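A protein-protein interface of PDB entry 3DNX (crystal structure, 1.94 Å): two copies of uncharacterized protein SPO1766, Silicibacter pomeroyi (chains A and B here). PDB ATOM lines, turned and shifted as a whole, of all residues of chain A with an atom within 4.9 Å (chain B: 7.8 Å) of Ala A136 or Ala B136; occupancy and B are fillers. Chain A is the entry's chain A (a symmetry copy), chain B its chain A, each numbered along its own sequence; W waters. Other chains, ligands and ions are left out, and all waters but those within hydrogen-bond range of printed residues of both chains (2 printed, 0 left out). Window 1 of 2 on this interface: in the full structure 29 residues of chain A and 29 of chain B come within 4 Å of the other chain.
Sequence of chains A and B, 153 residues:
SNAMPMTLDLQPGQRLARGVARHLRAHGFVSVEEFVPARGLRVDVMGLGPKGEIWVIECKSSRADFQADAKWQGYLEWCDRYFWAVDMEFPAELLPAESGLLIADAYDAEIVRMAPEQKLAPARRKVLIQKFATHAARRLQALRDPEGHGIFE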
ATOM      1  N   VAL A  32     -28.909 -27.634 -21.556  1.00  0.00           N
ATOM      2  CA  VAL A  32     -29.785 -28.225 -20.576  1.00  0.00           C
ATOM      3  C   VAL A  32     -31.215 -28.189 -21.109  1.00  0.00           C
ATOM      4  O   VAL A  32     -31.551 -27.431 -22.034  1.00  0.00           O
ATOM      5  CB  VAL A  32     -29.748 -27.554 -19.164  1.00  0.00           C
ATOM      6  CG1 VAL A  32     -28.333 -27.709 -18.523  1.00  0.00           C
ATOM      7  CG2 VAL A  32     -30.205 -26.122 -19.161  1.00  0.00           C
ATOM      8  N   PHE A 132     -27.882 -21.668 -15.432  1.00  0.00           N
ATOM      9  CA  PHE A 132     -27.575 -22.816 -16.255  1.00  0.00           C
ATOM     10  C   PHE A 132     -26.628 -23.774 -15.514  1.00  0.00           C
ATOM     11  O   PHE A 132     -26.905 -24.984 -15.420  1.00  0.00           O
ATOM     12  CB  PHE A 132     -26.968 -22.315 -17.550  1.00  0.00           C
ATOM     13  CG  PHE A 132     -26.594 -23.380 -18.516  1.00  0.00           C
ATOM     14  CD1 PHE A 132     -27.391 -23.633 -19.623  1.00  0.00           C
ATOM     15  CD2 PHE A 132     -25.426 -24.101 -18.379  1.00  0.00           C
ATOM     16  CE1 PHE A 132     -27.023 -24.598 -20.546  1.00  0.00           C
ATOM     17  CE2 PHE A 132     -25.056 -25.061 -19.293  1.00  0.00           C
ATOM     18  CZ  PHE A 132     -25.858 -25.337 -20.372  1.00  0.00           C
ATOM     19  N   ALA A 133     -25.534 -23.215 -14.997  1.00  0.00           N
ATOM     20  CA  ALA A 133     -24.550 -23.961 -14.150  1.00  0.00           C
ATOM     21  C   ALA A 133     -25.238 -24.717 -13.018  1.00  0.00           C
ATOM     22  O   ALA A 133     -25.059 -25.920 -12.814  1.00  0.00           O
ATOM     23  CB  ALA A 133     -23.521 -22.998 -13.561  1.00  0.00           C
ATOM     24  N   THR A 134     -26.076 -24.000 -12.317  1.00  0.00           N
ATOM     25  CA  THR A 134     -26.792 -24.566 -11.212  1.00  0.00           C
ATOM     26  C   THR A 134     -27.712 -25.688 -11.626  1.00  0.00           C
ATOM     27  O   THR A 134     -27.767 -26.711 -10.962  1.00  0.00           O
ATOM     28  CB  THR A 134     -27.560 -23.484 -10.489  1.00  0.00           C
ATOM     29  OG1 THR A 134     -26.605 -22.522 -10.034  1.00  0.00           O
ATOM     30  CG2 THR A 134     -28.298 -24.075  -9.305  1.00  0.00           C
ATOM     31  N   HIS A 135     -28.419 -25.490 -12.736  1.00  0.00           N
ATOM     32  CA  HIS A 135     -29.361 -26.478 -13.255  1.00  0.00           C
ATOM     33  C   HIS A 135     -28.612 -27.746 -13.631  1.00  0.00           C
ATOM     34  O   HIS A 135     -28.955 -28.873 -13.227  1.00  0.00           O
ATOM     35  CB  HIS A 135     -30.077 -25.852 -14.472  1.00  0.00           C
ATOM     36  CG  HIS A 135     -31.040 -26.751 -15.173  1.00  0.00           C
ATOM     37  ND1 HIS A 135     -32.357 -26.394 -15.383  1.00  0.00           N
ATOM     38  CD2 HIS A 135     -30.872 -27.946 -15.797  1.00  0.00           C
ATOM     39  CE1 HIS A 135     -32.964 -27.346 -16.074  1.00  0.00           C
ATOM     40  NE2 HIS A 135     -32.085 -28.297 -16.340  1.00  0.00           N
ATOM     41  N   ALA A 136     -27.578 -27.557 -14.439  1.00  0.00           N
ATOM     42  CA  ALA A 136     -26.787 -28.670 -14.906  1.00  0.00           C
ATOM     43  C   ALA A 136     -26.196 -29.482 -13.771  1.00  0.00           C
ATOM     44  O   ALA A 136     -26.238 -30.726 -13.787  1.00  0.00           O
ATOM     45  CB  ALA A 136     -25.692 -28.143 -15.797  1.00  0.00           C
ATOM     46  N   ALA A 137     -25.582 -28.797 -12.811  1.00  0.00           N
ATOM     47  CA  ALA A 137     -24.861 -29.480 -11.745  1.00  0.00           C
ATOM     48  C   ALA A 137     -25.817 -30.208 -10.786  1.00  0.00           C
ATOM     49  O   ALA A 137     -25.504 -31.308 -10.353  1.00  0.00           O
ATOM     50  CB  ALA A 137     -23.902 -28.546 -11.006  1.00  0.00           C
ATOM     51  N   ARG A 138     -26.996 -29.640 -10.522  1.00  0.00           N
ATOM     52  CA  ARG A 138     -28.001 -30.323  -9.703  1.00  0.00           C
ATOM     53  C   ARG A 138     -28.430 -31.621 -10.346  1.00  0.00           C
ATOM     54  O   ARG A 138     -28.446 -32.661  -9.702  1.00  0.00           O
ATOM     55  CB  ARG A 138     -29.259 -29.465  -9.462  1.00  0.00           C
ATOM     56  CG  ARG A 138     -29.151 -28.586  -8.283  1.00  0.00           C
ATOM     57  CD  ARG A 138     -30.492 -27.828  -7.991  1.00  0.00           C
ATOM     58  NE  ARG A 138     -30.248 -26.904  -6.876  1.00  0.00           N
ATOM     59  CZ  ARG A 138     -30.571 -25.601  -6.848  1.00  0.00           C
ATOM     60  NH1 ARG A 138     -31.225 -25.016  -7.864  1.00  0.00           N
ATOM     61  NH2 ARG A 138     -30.261 -24.878  -5.770  1.00  0.00           N
ATOM     62  N   ARG A 139     -28.843 -31.544 -11.626  1.00  0.00           N
ATOM     63  CA  ARG A 139     -29.314 -32.731 -12.332  1.00  0.00           C
ATOM     64  C   ARG A 139     -28.252 -33.794 -12.411  1.00  0.00           C
ATOM     65  O   ARG A 139     -28.549 -34.970 -12.327  1.00  0.00           O
ATOM     66  CB  ARG A 139     -29.761 -32.378 -13.769  1.00  0.00           C
ATOM     67  CG  ARG A 139     -30.791 -31.305 -13.852  1.00  0.00           C
ATOM     68  CD  ARG A 139     -32.107 -31.724 -13.403  1.00  0.00           C
ATOM     69  NE  ARG A 139     -33.112 -30.721 -13.792  1.00  0.00           N
ATOM     70  CZ  ARG A 139     -33.407 -29.603 -13.106  1.00  0.00           C
ATOM     71  NH1 ARG A 139     -32.769 -29.282 -11.975  1.00  0.00           N
ATOM     72  NH2 ARG A 139     -34.355 -28.794 -13.562  1.00  0.00           N
ATOM     73  N   LEU A 140     -27.020 -33.387 -12.667  1.00  0.00           N
ATOM     74  CA  LEU A 140     -25.891 -34.310 -12.707  1.00  0.00           C
ATOM     75  C   LEU A 140     -25.709 -35.037 -11.381  1.00  0.00           C
ATOM     76  O   LEU A 140     -25.628 -36.279 -11.330  1.00  0.00           O
ATOM     77  CB  LEU A 140     -24.633 -33.552 -13.059  1.00  0.00           C
ATOM     78  CG  LEU A 140     -23.287 -34.279 -13.057  1.00  0.00           C
ATOM     79  CD1 LEU A 140     -23.334 -35.536 -13.887  1.00  0.00           C
ATOM     80  CD2 LEU A 140     -22.236 -33.300 -13.547  1.00  0.00           C
ATOM     81  N   ARG B  25     -24.903 -29.383  -1.518  1.00  0.00           N
ATOM     82  CA  ARG B  25     -26.235 -29.267  -2.137  1.00  0.00           C
ATOM     83  C   ARG B  25     -27.316 -28.956  -1.068  1.00  0.00           C
ATOM     84  O   ARG B  25     -28.238 -28.142  -1.298  1.00  0.00           O
ATOM     85  CB  ARG B  25     -26.550 -30.501  -2.976  1.00  0.00           C
ATOM     86  CG  ARG B  25     -27.927 -30.490  -3.659  1.00  0.00           C
ATOM     87  CD  ARG B  25     -28.265 -31.803  -4.312  1.00  0.00           C
ATOM     88  NE  ARG B  25     -29.586 -31.635  -4.875  1.00  0.00           N
ATOM     89  CZ  ARG B  25     -29.968 -31.967  -6.104  1.00  0.00           C
ATOM     90  NH1 ARG B  25     -29.146 -32.591  -6.949  1.00  0.00           N
ATOM     91  NH2 ARG B  25     -31.216 -31.681  -6.470  1.00  0.00           N
ATOM     92  N   VAL B  30     -23.825 -26.001  -5.536  1.00  0.00           N
ATOM     93  CA  VAL B  30     -23.737 -27.127  -6.455  1.00  0.00           C
ATOM     94  C   VAL B  30     -22.254 -27.430  -6.644  1.00  0.00           C
ATOM     95  O   VAL B  30     -21.402 -26.633  -6.252  1.00  0.00           O
ATOM     96  CB  VAL B  30     -24.389 -26.819  -7.822  1.00  0.00           C
ATOM     97  CG1 VAL B  30     -25.953 -26.687  -7.648  1.00  0.00           C
ATOM     98  CG2 VAL B  30     -23.818 -25.541  -8.437  1.00  0.00           C
ATOM     99  N   SER B  31     -21.950 -28.534  -7.282  1.00  0.00           N
ATOM    100  CA  SER B  31     -20.553 -28.966  -7.362  1.00  0.00           C
ATOM    101  C   SER B  31     -20.315 -29.801  -8.601  1.00  0.00           C
ATOM    102  O   SER B  31     -21.248 -30.347  -9.201  1.00  0.00           O
ATOM    103  CB  SER B  31     -20.145 -29.717  -6.123  1.00  0.00           C
ATOM    104  OG  SER B  31     -20.900 -30.926  -5.986  1.00  0.00           O
ATOM    105  N   VAL B  32     -19.038 -29.870  -8.980  1.00  0.00           N
ATOM    106  CA  VAL B  32     -18.558 -30.845  -9.928  1.00  0.00           C
ATOM    107  C   VAL B  32     -17.277 -31.472  -9.382  1.00  0.00           C
ATOM    108  O   VAL B  32     -16.612 -30.930  -8.485  1.00  0.00           O
ATOM    109  CB  VAL B  32     -18.285 -30.293 -11.365  1.00  0.00           C
ATOM    110  CG1 VAL B  32     -19.610 -29.781 -12.014  1.00  0.00           C
ATOM    111  CG2 VAL B  32     -17.202 -29.253 -11.420  1.00  0.00           C
ATOM    112  N   GLU B  33     -16.934 -32.604  -9.955  1.00  0.00           N
ATOM    113  CA  GLU B  33     -15.718 -33.273  -9.603  1.00  0.00           C
ATOM    114  C   GLU B  33     -14.645 -33.202 -10.692  1.00  0.00           C
ATOM    115  O   GLU B  33     -14.927 -33.097 -11.900  1.00  0.00           O
ATOM    116  CB  GLU B  33     -16.013 -34.741  -9.281  1.00  0.00           C
ATOM    117  CG  GLU B  33     -16.655 -34.996  -7.961  1.00  0.00           C
ATOM    118  CD  GLU B  33     -16.685 -36.509  -7.615  1.00  0.00           C
ATOM    119  OE1 GLU B  33     -15.614 -37.208  -7.697  1.00  0.00           O
ATOM    120  OE2 GLU B  33     -17.767 -36.999  -7.230  1.00  0.00           O
ATOM    121  N   PHE B  35     -12.351 -30.943 -11.538  1.00  0.00           N
ATOM    122  CA  PHE B  35     -12.405 -29.728 -12.284  1.00  0.00           C
ATOM    123  C   PHE B  35     -11.030 -29.128 -12.627  1.00  0.00           C
ATOM    124  O   PHE B  35     -10.160 -29.024 -11.755  1.00  0.00           O
ATOM    125  CB  PHE B  35     -13.161 -28.703 -11.486  1.00  0.00           C
ATOM    126  CG  PHE B  35     -13.334 -27.433 -12.199  1.00  0.00           C
ATOM    127  CD1 PHE B  35     -12.605 -26.328 -11.833  1.00  0.00           C
ATOM    128  CD2 PHE B  35     -14.201 -27.344 -13.277  1.00  0.00           C
ATOM    129  CE1 PHE B  35     -12.760 -25.135 -12.478  1.00  0.00           C
ATOM    130  CE2 PHE B  35     -14.333 -26.151 -13.944  1.00  0.00           C
ATOM    131  CZ  PHE B  35     -13.624 -25.034 -13.534  1.00  0.00           C
ATOM    132  N   ILE B 129     -16.779 -19.910 -13.901  1.00  0.00           N
ATOM    133  CA  ILE B 129     -18.203 -20.271 -13.961  1.00  0.00           C
ATOM    134  C   ILE B 129     -18.599 -20.862 -15.324  1.00  0.00           C
ATOM    135  O   ILE B 129     -19.369 -21.843 -15.399  1.00  0.00           O
ATOM    136  CB  ILE B 129     -19.123 -19.096 -13.512  1.00  0.00           C
ATOM    137  CG1 ILE B 129     -18.811 -18.772 -12.039  1.00  0.00           C
ATOM    138  CG2 ILE B 129     -20.662 -19.441 -13.772  1.00  0.00           C
ATOM    139  CD1 ILE B 129     -19.682 -17.732 -11.416  1.00  0.00           C
ATOM    140  N   GLN B 130     -18.018 -20.326 -16.382  1.00  0.00           N
ATOM    141  CA  GLN B 130     -18.248 -20.816 -17.737  1.00  0.00           C
ATOM    142  C   GLN B 130     -17.722 -22.247 -17.868  1.00  0.00           C
ATOM    143  O   GLN B 130     -18.379 -23.123 -18.485  1.00  0.00           O
ATOM    144  CB  GLN B 130     -17.591 -19.891 -18.776  1.00  0.00           C
ATOM    145  CG  GLN B 130     -17.528 -20.435 -20.192  1.00  0.00           C
ATOM    146  CD  GLN B 130     -18.822 -20.317 -20.893  1.00  0.00           C
ATOM    147  OE1 GLN B 130     -19.507 -19.307 -20.754  1.00  0.00           O
ATOM    148  NE2 GLN B 130     -19.159 -21.318 -21.711  1.00  0.00           N
ATOM    149  N   LYS B 131     -16.554 -22.481 -17.267  1.00  0.00           N
ATOM    150  CA  LYS B 131     -15.907 -23.791 -17.313  1.00  0.00           C
ATOM    151  C   LYS B 131     -16.697 -24.803 -16.513  1.00  0.00           C
ATOM    152  O   LYS B 131     -16.847 -25.937 -16.933  1.00  0.00           O
ATOM    153  CB  LYS B 131     -14.480 -23.712 -16.781  1.00  0.00           C
ATOM    154  CG  LYS B 131     -13.499 -23.187 -17.779  1.00  0.00           C
ATOM    155  CD  LYS B 131     -12.106 -22.993 -17.185  1.00  0.00           C
ATOM    156  CE  LYS B 131     -11.293 -22.104 -18.134  1.00  0.00           C
ATOM    157  NZ  LYS B 131      -9.911 -22.657 -18.341  1.00  0.00           N
ATOM    158  N   PHE B 132     -17.163 -24.381 -15.345  1.00  0.00           N
ATOM    159  CA  PHE B 132     -17.971 -25.211 -14.480  1.00  0.00           C
ATOM    160  C   PHE B 132     -19.267 -25.631 -15.193  1.00  0.00           C
ATOM    161  O   PHE B 132     -19.601 -26.830 -15.236  1.00  0.00           O
ATOM    162  CB  PHE B 132     -18.254 -24.431 -13.213  1.00  0.00           C
ATOM    163  CG  PHE B 132     -19.080 -25.151 -12.209  1.00  0.00           C
ATOM    164  CD1 PHE B 132     -18.487 -25.708 -11.085  1.00  0.00           C
ATOM    165  CD2 PHE B 132     -20.451 -25.234 -12.329  1.00  0.00           C
ATOM    166  CE1 PHE B 132     -19.261 -26.344 -10.128  1.00  0.00           C
ATOM    167  CE2 PHE B 132     -21.224 -25.865 -11.382  1.00  0.00           C
ATOM    168  CZ  PHE B 132     -20.640 -26.446 -10.285  1.00  0.00           C
ATOM    169  N   ALA B 133     -19.968 -24.641 -15.742  1.00  0.00           N
ATOM    170  CA  ALA B 133     -21.197 -24.861 -16.569  1.00  0.00           C
ATOM    171  C   ALA B 133     -20.963 -25.897 -17.663  1.00  0.00           C
ATOM    172  O   ALA B 133     -21.695 -26.877 -17.821  1.00  0.00           O
ATOM    173  CB  ALA B 133     -21.650 -23.548 -17.206  1.00  0.00           C
ATOM    174  N   THR B 134     -19.892 -25.694 -18.383  1.00  0.00           N
ATOM    175  CA  THR B 134     -19.543 -26.576 -19.458  1.00  0.00           C
ATOM    176  C   THR B 134     -19.264 -27.983 -18.992  1.00  0.00           C
ATOM    177  O   THR B 134     -19.708 -28.934 -19.613  1.00  0.00           O
ATOM    178  CB  THR B 134     -18.360 -26.018 -20.216  1.00  0.00           C
ATOM    179  OG1 THR B 134     -18.747 -24.737 -20.718  1.00  0.00           O
ATOM    180  CG2 THR B 134     -18.004 -26.936 -21.368  1.00  0.00           C
ATOM    181  N   HIS B 135     -18.537 -28.101 -17.883  1.00  0.00           N
ATOM    182  CA  HIS B 135     -18.172 -29.397 -17.316  1.00  0.00           C
ATOM    183  C   HIS B 135     -19.431 -30.140 -16.898  1.00  0.00           C
ATOM    184  O   HIS B 135     -19.669 -31.309 -17.253  1.00  0.00           O
ATOM    185  CB  HIS B 135     -17.233 -29.140 -16.117  1.00  0.00           C
ATOM    186  CG  HIS B 135     -16.807 -30.360 -15.372  1.00  0.00           C
ATOM    187  ND1 HIS B 135     -15.476 -30.665 -15.163  1.00  0.00           N
ATOM    188  CD2 HIS B 135     -17.517 -31.306 -14.703  1.00  0.00           C
ATOM    189  CE1 HIS B 135     -15.389 -31.763 -14.429  1.00  0.00           C
ATOM    190  NE2 HIS B 135     -16.612 -32.170 -14.135  1.00  0.00           N
ATOM    191  N   ALA B 136     -20.243 -29.450 -16.108  1.00  0.00           N
ATOM    192  CA  ALA B 136     -21.463 -30.033 -15.605  1.00  0.00           C
ATOM    193  C   ALA B 136     -22.381 -30.510 -16.713  1.00  0.00           C
ATOM    194  O   ALA B 136     -22.935 -31.623 -16.647  1.00  0.00           O
ATOM    195  CB  ALA B 136     -22.167 -29.014 -14.747  1.00  0.00           C
ATOM    196  N   ALA B 137     -22.605 -29.654 -17.705  1.00  0.00           N
ATOM    197  CA  ALA B 137     -23.574 -29.954 -18.751  1.00  0.00           C
ATOM    198  C   ALA B 137     -23.089 -31.086 -19.671  1.00  0.00           C
ATOM    199  O   ALA B 137     -23.892 -31.921 -20.063  1.00  0.00           O
ATOM    200  CB  ALA B 137     -23.980 -28.706 -19.536  1.00  0.00           C
ATOM    201  N   ARG B 138     -21.785 -31.158 -19.945  1.00  0.00           N
ATOM    202  CA  ARG B 138     -21.234 -32.269 -20.727  1.00  0.00           C
ATOM    203  C   ARG B 138     -21.468 -33.588 -20.028  1.00  0.00           C
ATOM    204  O   ARG B 138     -21.955 -34.535 -20.631  1.00  0.00           O
ATOM    205  CB  ARG B 138     -19.722 -32.123 -20.988  1.00  0.00           C
ATOM    206  CG  ARG B 138     -19.410 -31.346 -22.203  1.00  0.00           C
ATOM    207  CD  ARG B 138     -17.873 -31.329 -22.511  1.00  0.00           C
ATOM    208  NE  ARG B 138     -17.660 -30.446 -23.664  1.00  0.00           N
ATOM    209  CZ  ARG B 138     -16.755 -29.456 -23.740  1.00  0.00           C
ATOM    210  NH1 ARG B 138     -15.892 -29.213 -22.741  1.00  0.00           N
ATOM    211  NH2 ARG B 138     -16.695 -28.716 -24.849  1.00  0.00           N
ATOM    212  N   ARG B 139     -21.055 -33.666 -18.748  1.00  0.00           N
ATOM    213  CA  ARG B 139     -21.199 -34.906 -17.992  1.00  0.00           C
ATOM    214  C   ARG B 139     -22.638 -35.331 -17.881  1.00  0.00           C
ATOM    215  O   ARG B 139     -22.937 -36.509 -17.916  1.00  0.00           O
ATOM    216  CB  ARG B 139     -20.623 -34.751 -16.565  1.00  0.00           C
ATOM    217  CG  ARG B 139     -19.206 -34.295 -16.514  1.00  0.00           C
ATOM    218  CD  ARG B 139     -18.252 -35.307 -16.933  1.00  0.00           C
ATOM    219  NE  ARG B 139     -16.888 -34.889 -16.574  1.00  0.00           N
ATOM    220  CZ  ARG B 139     -16.103 -34.074 -17.300  1.00  0.00           C
ATOM    221  NH1 ARG B 139     -16.523 -33.533 -18.450  1.00  0.00           N
ATOM    222  NH2 ARG B 139     -14.880 -33.796 -16.867  1.00  0.00           N
ATOM    223  N   LEU B 140     -23.525 -34.377 -17.653  1.00  0.00           N
ATOM    224  CA  LEU B 140     -24.956 -34.649 -17.589  1.00  0.00           C
ATOM    225  C   LEU B 140     -25.476 -35.254 -18.887  1.00  0.00           C
ATOM    226  O   LEU B 140     -26.139 -36.309 -18.889  1.00  0.00           O
ATOM    227  CB  LEU B 140     -25.699 -33.370 -17.280  1.00  0.00           C
ATOM    228  CG  LEU B 140     -27.229 -33.369 -17.266  1.00  0.00           C
ATOM    229  CD1 LEU B 140     -27.777 -34.463 -16.387  1.00  0.00           C
ATOM    230  CD2 LEU B 140     -27.682 -31.990 -16.826  1.00  0.00           C
ATOM    231  N   GLN B 141     -25.145 -34.613 -20.010  1.00  0.00           N
ATOM    232  CA  GLN B 141     -25.598 -35.116 -21.305  1.00  0.00           C
ATOM    233  C   GLN B 141     -25.086 -36.547 -21.577  1.00  0.00           C
ATOM    234  O   GLN B 141     -25.812 -37.366 -22.103  1.00  0.00           O
ATOM    235  CB  GLN B 141     -25.263 -34.138 -22.445  1.00  0.00           C
ATOM    236  CG  GLN B 141     -25.960 -34.467 -23.800  1.00  0.00           C
ATOM    237  CD  GLN B 141     -25.098 -35.360 -24.676  1.00  0.00           C
ATOM    238  OE1 GLN B 141     -23.961 -35.702 -24.285  1.00  0.00           O
ATOM    239  NE2 GLN B 141     -25.620 -35.765 -25.844  1.00  0.00           N
ATOM    240  N   ALA B 142     -23.846 -36.824 -21.209  1.00  0.00           N
ATOM    241  CA  ALA B 142     -23.263 -38.121 -21.402  1.00  0.00           C
ATOM    242  C   ALA B 142     -23.939 -39.229 -20.547  1.00  0.00           C
ATOM    243  O   ALA B 142     -23.992 -40.390 -20.970  1.00  0.00           O
ATOM    244  CB  ALA B 142     -21.782 -38.049 -21.144  1.00  0.00           C
HETATM  245  O   HOH W   1     -22.769 -32.325 -10.196  1.00  0.00           O
HETATM  246  O   HOH W   2     -24.637 -30.155  -7.519  1.00  0.00           O
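Phe A132 touches Ala B133, and with the chains exchanged Ala A133 touches Phe B132.
Phe A132 touches Ala B137, and with the chains exchanged Ala A137 touches Phe B132.
Ala A136 touches Leu B140, and with the chains exchanged Leu A140 touches Ala B136.
Arg A139 touches Leu B140, and with the chains exchanged Leu A140 touches Arg B139.
Among the printed residues, pairs that only touch across the chains: Phe A132 with Ala B133 (3.99 Å), Phe A132 with Ala B137 (3.8 Å), Ala A133 with Phe B132 (3.99 Å), Thr A134 with Val B30 (3.8 Å), Ala A136 with Ala B136 (3.8 Å), Ala A136 with Ala B137 (3.9 Å), Ala A136 with Leu B140 (3.6 Å), Ala A137 with Val B30 (3.7 Å), Ala A137 with Ser B31 (3.7 Å), Ala A137 with Phe B132 (3.8 Å), Ala A137 with Ala B136 (3.9 Å), Arg A138 with Val B30 (3.8 Å), Arg A139 with Leu B140 (3.7 Å), Leu A140 with Ala B136 (3.6 Å), Leu A140 with Arg B139 (3.7 Å) and Leu A140 with Leu B140 (3.9 Å).
Hydrophobic or aromatic side chains of chain A within 4 Å of the printed part of chain B: Phe A132, Ala A133, Ala A136, Ala A137 and Leu A140.
Of the 20 printed residues of chain B, 9 touch a printed residue of chain A.
Hydrophobic or aromatic side chains of chain B that line the printed part of chain A: Val B30, Phe B132, Ala B133, Ala B136, Ala B137 and Leu B140.
Among the printed residues, 17 pairs touch across the chains.
Among the printed residues, no Asp or Glu carboxylate lies within 4 Å of a Lys or Arg side-chain nitrogen of the other chain.
Ala B136 touches three residues of chain A.
Of chain B, only Val B30 (3.7 Å), Ser B31 (3.7 Å), Phe B132 (3.8 Å) and Ala B136 (3.9 Å) come within 4 Å of Ala A137.
Of the printed residues of chain B, Ala A133 touches Phe B132 (3.99 Å).
Of the printed residues of chain A, Leu B140 touches Ala A136, Arg A139 and Leu A140.
Of the printed residues of chain B, Arg A139 touches Leu B140 (3.7 Å).
His A135 touches none of the printed residues of chain B.
Ala B142 touches none of the printed residues of chain A.
The nearest residue of chain B that does not touch Ala A136 is Ala B133 (4.7 Å).
The nearest printed residue of chain B that does not touch Ala A133 is Ala B133 (4.1 Å).
Water W1 lies within hydrogen-bond range of the backbone carbonyl oxygen of Ser B31 (2.7 Å) and the backbone carbonyl oxygen of Ala A137 (2.9 Å).
Water W2 bridges the backbone NH (N) of Ser B31 (3.1 Å) and the backbone carbonyl oxygen (O) of Ala A137 (3.2 Å).
NH1 of Arg B25 sits at hydrogen-bond distance from O of Arg A138 (2.8 Å).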
